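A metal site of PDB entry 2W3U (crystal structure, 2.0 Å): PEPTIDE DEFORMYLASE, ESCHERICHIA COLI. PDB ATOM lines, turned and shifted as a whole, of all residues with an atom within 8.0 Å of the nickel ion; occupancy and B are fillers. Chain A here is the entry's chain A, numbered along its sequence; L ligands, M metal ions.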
ATOM      1  N   VAL A   5     -33.733   3.885 -14.819  1.00  0.00           N
ATOM      2  CA  VAL A   5     -32.651   4.338 -13.955  1.00  0.00           C
ATOM      3  C   VAL A   5     -32.895   5.785 -13.564  1.00  0.00           C
ATOM      4  O   VAL A   5     -32.907   6.673 -14.398  1.00  0.00           O
ATOM      5  CB  VAL A   5     -31.282   4.251 -14.638  1.00  0.00           C
ATOM      6  CG1 VAL A   5     -30.161   4.766 -13.714  1.00  0.00           C
ATOM      7  CG2 VAL A   5     -31.011   2.832 -15.079  1.00  0.00           C
ATOM      8  N   LEU A  13     -32.602   8.620  -4.908  1.00  0.00           N
ATOM      9  CA  LEU A  13     -31.198   8.178  -5.002  1.00  0.00           C
ATOM     10  C   LEU A  13     -30.428   8.350  -3.696  1.00  0.00           C
ATOM     11  O   LEU A  13     -29.341   7.797  -3.528  1.00  0.00           O
ATOM     12  CB  LEU A  13     -30.481   8.898  -6.144  1.00  0.00           C
ATOM     13  CG  LEU A  13     -30.743   8.412  -7.578  1.00  0.00           C
ATOM     14  CD1 LEU A  13     -30.153   9.393  -8.562  1.00  0.00           C
ATOM     15  CD2 LEU A  13     -30.206   7.001  -7.825  1.00  0.00           C
ATOM     16  N   GLY A  45     -21.885  -1.490 -13.656  1.00  0.00           N
ATOM     17  CA  GLY A  45     -22.399  -1.676 -12.310  1.00  0.00           C
ATOM     18  C   GLY A  45     -23.762  -1.048 -12.185  1.00  0.00           C
ATOM     19  O   GLY A  45     -24.069  -0.080 -12.889  1.00  0.00           O
ATOM     20  N   LEU A  46     -24.580  -1.574 -11.289  1.00  0.00           N
ATOM     21  CA  LEU A  46     -25.875  -0.985 -10.987  1.00  0.00           C
ATOM     22  C   LEU A  46     -26.310  -1.418  -9.600  1.00  0.00           C
ATOM     23  O   LEU A  46     -26.184  -2.578  -9.245  1.00  0.00           O
ATOM     24  CB  LEU A  46     -26.948  -1.440 -11.999  1.00  0.00           C
ATOM     25  CG  LEU A  46     -28.345  -0.845 -11.818  1.00  0.00           C
ATOM     26  CD1 LEU A  46     -28.358   0.615 -12.289  1.00  0.00           C
ATOM     27  CD2 LEU A  46     -29.440  -1.706 -12.542  1.00  0.00           C
ATOM     28  N   ALA A  47     -26.819  -0.463  -8.830  1.00  0.00           N
ATOM     29  CA  ALA A  47     -27.302  -0.759  -7.490  1.00  0.00           C
ATOM     30  C   ALA A  47     -28.811  -0.641  -7.518  1.00  0.00           C
ATOM     31  O   ALA A  47     -29.338   0.127  -8.324  1.00  0.00           O
ATOM     32  CB  ALA A  47     -26.707   0.218  -6.476  1.00  0.00           C
ATOM     33  N   GLN A  50     -30.734   2.610  -7.529  1.00  0.00           N
ATOM     34  CA  GLN A  50     -30.794   3.346  -8.780  1.00  0.00           C
ATOM     35  C   GLN A  50     -32.055   3.051  -9.574  1.00  0.00           C
ATOM     36  O   GLN A  50     -32.519   3.908 -10.325  1.00  0.00           O
ATOM     37  CB  GLN A  50     -29.557   3.072  -9.640  1.00  0.00           C
ATOM     38  CG  GLN A  50     -28.323   3.844  -9.213  1.00  0.00           C
ATOM     39  CD  GLN A  50     -27.090   3.330  -9.920  1.00  0.00           C
ATOM     40  OE1 GLN A  50     -26.576   2.252  -9.620  1.00  0.00           O
ATOM     41  NE2 GLN A  50     -26.628   4.090 -10.910  1.00  0.00           N
ATOM     42  N   GLU A  88     -14.657   8.424 -12.826  1.00  0.00           N
ATOM     43  CA  GLU A  88     -15.794   7.540 -12.726  1.00  0.00           C
ATOM     44  C   GLU A  88     -17.035   8.123 -13.412  1.00  0.00           C
ATOM     45  O   GLU A  88     -17.249   9.335 -13.349  1.00  0.00           O
ATOM     46  CB  GLU A  88     -16.132   7.292 -11.243  1.00  0.00           C
ATOM     47  CG  GLU A  88     -15.102   6.468 -10.485  1.00  0.00           C
ATOM     48  CD  GLU A  88     -15.515   6.149  -9.059  1.00  0.00           C
ATOM     49  OE1 GLU A  88     -16.738   6.160  -8.776  1.00  0.00           O
ATOM     50  OE2 GLU A  88     -14.617   5.947  -8.202  1.00  0.00           O
ATOM     51  N   GLY A  89     -17.836   7.256 -14.022  1.00  0.00           N
ATOM     52  CA  GLY A  89     -19.128   7.647 -14.597  1.00  0.00           C
ATOM     53  C   GLY A  89     -20.216   7.063 -13.709  1.00  0.00           C
ATOM     54  O   GLY A  89     -19.915   6.390 -12.728  1.00  0.00           O
ATOM     55  N   CYS A  90     -21.469   7.339 -14.023  1.00  0.00           N
ATOM     56  CA  CYS A  90     -22.574   6.813 -13.236  1.00  0.00           C
ATOM     57  C   CYS A  90     -23.828   6.929 -14.071  1.00  0.00           C
ATOM     58  O   CYS A  90     -24.128   7.998 -14.620  1.00  0.00           O
ATOM     59  CB  CYS A  90     -22.753   7.560 -11.911  1.00  0.00           C
ATOM     60  SG  CYS A  90     -24.086   6.875 -10.857  1.00  0.00           S
ATOM     61  N   LEU A  91     -24.550   5.808 -14.191  1.00  0.00           N
ATOM     62  CA  LEU A  91     -25.777   5.804 -14.992  1.00  0.00           C
ATOM     63  C   LEU A  91     -26.814   6.747 -14.393  1.00  0.00           C
ATOM     64  O   LEU A  91     -27.735   7.159 -15.073  1.00  0.00           O
ATOM     65  CB  LEU A  91     -26.314   4.364 -15.189  1.00  0.00           C
ATOM     66  CG  LEU A  91     -25.270   3.418 -15.801  1.00  0.00           C
ATOM     67  CD1 LEU A  91     -25.527   1.913 -15.541  1.00  0.00           C
ATOM     68  CD2 LEU A  91     -25.116   3.705 -17.307  1.00  0.00           C
ATOM     69  N   SER A  92     -26.653   7.138 -13.119  1.00  0.00           N
ATOM     70  CA  SER A  92     -27.572   8.116 -12.506  1.00  0.00           C
ATOM     71  C   SER A  92     -27.132   9.562 -12.722  1.00  0.00           C
ATOM     72  O   SER A  92     -27.841  10.500 -12.368  1.00  0.00           O
ATOM     73  CB  SER A  92     -27.756   7.834 -11.014  1.00  0.00           C
ATOM     74  OG  SER A  92     -28.662   6.755 -10.824  1.00  0.00           O
ATOM     75  N   ILE A  93     -25.954   9.719 -13.322  1.00  0.00           N
ATOM     76  CA  ILE A  93     -25.367  11.027 -13.580  1.00  0.00           C
ATOM     77  C   ILE A  93     -24.848  11.054 -15.038  1.00  0.00           C
ATOM     78  O   ILE A  93     -23.636  11.107 -15.270  1.00  0.00           O
ATOM     79  CB  ILE A  93     -24.239  11.379 -12.558  1.00  0.00           C
ATOM     80  CG1 ILE A  93     -24.651  11.057 -11.116  1.00  0.00           C
ATOM     81  CG2 ILE A  93     -23.874  12.855 -12.689  1.00  0.00           C
ATOM     82  CD1 ILE A  93     -23.527  11.259 -10.051  1.00  0.00           C
ATOM     83  N   ARG A 102     -10.544   6.494  -3.870  1.00  0.00           N
ATOM     84  CA  ARG A 102     -11.067   5.160  -3.567  1.00  0.00           C
ATOM     85  C   ARG A 102      -9.924   4.377  -2.974  1.00  0.00           C
ATOM     86  O   ARG A 102      -8.736   4.670  -3.251  1.00  0.00           O
ATOM     87  CB  ARG A 102     -11.540   4.419  -4.854  1.00  0.00           C
ATOM     88  CG  ARG A 102     -12.685   5.107  -5.624  1.00  0.00           C
ATOM     89  CD  ARG A 102     -14.020   4.992  -4.820  1.00  0.00           C
ATOM     90  NE  ARG A 102     -15.139   5.505  -5.600  1.00  0.00           N
ATOM     91  CZ  ARG A 102     -16.368   5.679  -5.135  1.00  0.00           C
ATOM     92  NH1 ARG A 102     -16.643   5.370  -3.863  1.00  0.00           N
ATOM     93  NH2 ARG A 102     -17.327   6.183  -5.950  1.00  0.00           N
ATOM     94  N   CYS A 129     -15.327  -0.088  -8.846  1.00  0.00           N
ATOM     95  CA  CYS A 129     -16.729  -0.317  -9.171  1.00  0.00           C
ATOM     96  C   CYS A 129     -17.512  -0.831  -7.942  1.00  0.00           C
ATOM     97  O   CYS A 129     -18.641  -0.373  -7.636  1.00  0.00           O
ATOM     98  CB  CYS A 129     -16.841  -1.404 -10.246  1.00  0.00           C
ATOM     99  SG  CYS A 129     -18.518  -1.588 -10.862  1.00  0.00           S
ATOM    100  N   HIS A 132     -18.050   2.138  -5.573  1.00  0.00           N
ATOM    101  CA  HIS A 132     -19.025   3.066  -6.203  1.00  0.00           C
ATOM    102  C   HIS A 132     -20.432   2.503  -6.026  1.00  0.00           C
ATOM    103  O   HIS A 132     -21.348   3.244  -5.617  1.00  0.00           O
ATOM    104  CB  HIS A 132     -18.679   3.178  -7.689  1.00  0.00           C
ATOM    105  CG  HIS A 132     -19.677   3.949  -8.515  1.00  0.00           C
ATOM    106  ND1 HIS A 132     -19.392   5.202  -9.013  1.00  0.00           N
ATOM    107  CD2 HIS A 132     -20.908   3.628  -8.994  1.00  0.00           C
ATOM    108  CE1 HIS A 132     -20.408   5.635  -9.741  1.00  0.00           C
ATOM    109  NE2 HIS A 132     -21.351   4.698  -9.738  1.00  0.00           N
ATOM    110  N   GLU A 133     -20.608   1.203  -6.321  1.00  0.00           N
ATOM    111  CA  GLU A 133     -21.926   0.551  -6.169  1.00  0.00           C
ATOM    112  C   GLU A 133     -22.397   0.430  -4.723  1.00  0.00           C
ATOM    113  O   GLU A 133     -23.568   0.683  -4.426  1.00  0.00           O
ATOM    114  CB  GLU A 133     -22.014  -0.795  -6.915  1.00  0.00           C
ATOM    115  CG  GLU A 133     -21.832  -0.717  -8.454  1.00  0.00           C
ATOM    116  CD  GLU A 133     -22.735   0.319  -9.108  1.00  0.00           C
ATOM    117  OE1 GLU A 133     -23.840   0.537  -8.581  1.00  0.00           O
ATOM    118  OE2 GLU A 133     -22.348   0.918 -10.134  1.00  0.00           O
ATOM    119  N   ASP A 135     -21.583   2.475  -2.427  1.00  0.00           N
ATOM    120  CA  ASP A 135     -21.947   3.860  -2.037  1.00  0.00           C
ATOM    121  C   ASP A 135     -23.409   4.131  -2.367  1.00  0.00           C
ATOM    122  O   ASP A 135     -24.134   4.758  -1.578  1.00  0.00           O
ATOM    123  CB  ASP A 135     -21.065   4.900  -2.740  1.00  0.00           C
ATOM    124  CG  ASP A 135     -19.807   5.251  -1.961  1.00  0.00           C
ATOM    125  OD1 ASP A 135     -19.610   4.778  -0.821  1.00  0.00           O
ATOM    126  OD2 ASP A 135     -18.993   6.028  -2.505  1.00  0.00           O
ATOM    127  N   HIS A 136     -23.850   3.636  -3.538  1.00  0.00           N
ATOM    128  CA  HIS A 136     -25.239   3.776  -3.963  1.00  0.00           C
ATOM    129  C   HIS A 136     -26.246   3.270  -2.951  1.00  0.00           C
ATOM    130  O   HIS A 136     -27.304   3.860  -2.812  1.00  0.00           O
ATOM    131  CB  HIS A 136     -25.493   3.052  -5.279  1.00  0.00           C
ATOM    132  CG  HIS A 136     -25.172   3.866  -6.492  1.00  0.00           C
ATOM    133  ND1 HIS A 136     -25.675   5.129  -6.695  1.00  0.00           N
ATOM    134  CD2 HIS A 136     -24.402   3.585  -7.567  1.00  0.00           C
ATOM    135  CE1 HIS A 136     -25.240   5.591  -7.850  1.00  0.00           C
ATOM    136  NE2 HIS A 136     -24.459   4.672  -8.398  1.00  0.00           N
ATOM    137  N   LYS A 140     -25.187   7.372  -1.454  1.00  0.00           N
ATOM    138  CA  LYS A 140     -24.048   8.211  -1.742  1.00  0.00           C
ATOM    139  C   LYS A 140     -23.645   8.158  -3.226  1.00  0.00           C
ATOM    140  O   LYS A 140     -23.718   7.106  -3.860  1.00  0.00           O
ATOM    141  CB  LYS A 140     -22.880   7.840  -0.798  1.00  0.00           C
ATOM    142  CG  LYS A 140     -21.600   8.615  -1.029  1.00  0.00           C
ATOM    143  CD  LYS A 140     -20.734   8.764   0.256  1.00  0.00           C
ATOM    144  CE  LYS A 140     -20.344   7.415   0.835  1.00  0.00           C
ATOM    145  NZ  LYS A 140     -19.581   7.545   2.101  1.00  0.00           N
ATOM    146  N   LEU A 141     -23.220   9.288  -3.780  1.00  0.00           N
ATOM    147  CA  LEU A 141     -22.897   9.412  -5.217  1.00  0.00           C
ATOM    148  C   LEU A 141     -21.469   9.909  -5.415  1.00  0.00           C
ATOM    149  O   LEU A 141     -20.920  10.572  -4.514  1.00  0.00           O
ATOM    150  CB  LEU A 141     -23.888  10.356  -5.890  1.00  0.00           C
ATOM    151  CG  LEU A 141     -25.359   9.954  -5.814  1.00  0.00           C
ATOM    152  CD1 LEU A 141     -26.278  11.147  -6.058  1.00  0.00           C
ATOM    153  CD2 LEU A 141     -25.671   8.855  -6.795  1.00  0.00           C
ATOM    154  N   PHE A 142     -20.863   9.615  -6.563  1.00  0.00           N
ATOM    155  CA  PHE A 142     -19.430   9.932  -6.748  1.00  0.00           C
ATOM    156  C   PHE A 142     -19.211  11.463  -6.633  1.00  0.00           C
ATOM    157  O   PHE A 142     -18.151  11.925  -6.140  1.00  0.00           O
ATOM    158  CB  PHE A 142     -18.824   9.298  -8.021  1.00  0.00           C
ATOM    159  CG  PHE A 142     -19.155  10.068  -9.319  1.00  0.00           C
ATOM    160  CD1 PHE A 142     -18.386  11.151  -9.710  1.00  0.00           C
ATOM    161  CD2 PHE A 142     -20.176   9.638 -10.161  1.00  0.00           C
ATOM    162  CE1 PHE A 142     -18.670  11.867 -10.885  1.00  0.00           C
ATOM    163  CE2 PHE A 142     -20.465  10.305 -11.343  1.00  0.00           C
ATOM    164  CZ  PHE A 142     -19.712  11.424 -11.710  1.00  0.00           C
HETATM  165  C1  LIG L   1     -23.941   3.103 -12.217  1.00  0.00           C
HETATM  166  O1  LIG L   1     -24.046   3.309 -11.022  1.00  0.00           O
HETATM  167  O2  LIG L   1     -22.877   3.254 -12.805  1.00  0.00           O
HETATM  168 NI    NI M   1     -23.356   4.972 -10.090  1.00  0.00          NI
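NE2 of His 136 lies close to NE2 of Gln 50 (3.4 Å).
OE1 of Glu 88 lies within hydrogen-bond range of ND1 of His 132, at 2.8 Å.
The side-chain amide nitrogen (NE2) of Gln 50 lies close to the side-chain sulfur (SG) of Cys 90 (3.8 Å).
The backbone NH (N) of Ser 92 sits close to the side-chain sulfur (SG) of Cys 90.
The side-chain amide oxygen (OE1) of Gln 50 lies close to the side-chain carboxylate (OE1) of Glu 133, at 3.4 Å.
NE2 of Gln 50 lies close to OG of Ser 92 (3.4 Å).
OE1 of Gln 50 sits at hydrogen-bond distance from N of Ala 47 (2.8 Å).
Gln 50 touches the nickel ion.
Of the 21 residues printed, 4 come within 4 Å of the nickel ion.
The nickel ion is bound by O1 of the ligand.
NE2 of His 136 binds the nickel ion (2.0 Å).
The nickel ion is bound by NE2 of His 132 (2.1 Å).
The nickel ion is bound by the side-chain sulfur (SG) of Cys 90 (2.2 Å).
The nickel ion has four donor atoms within binding distance.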
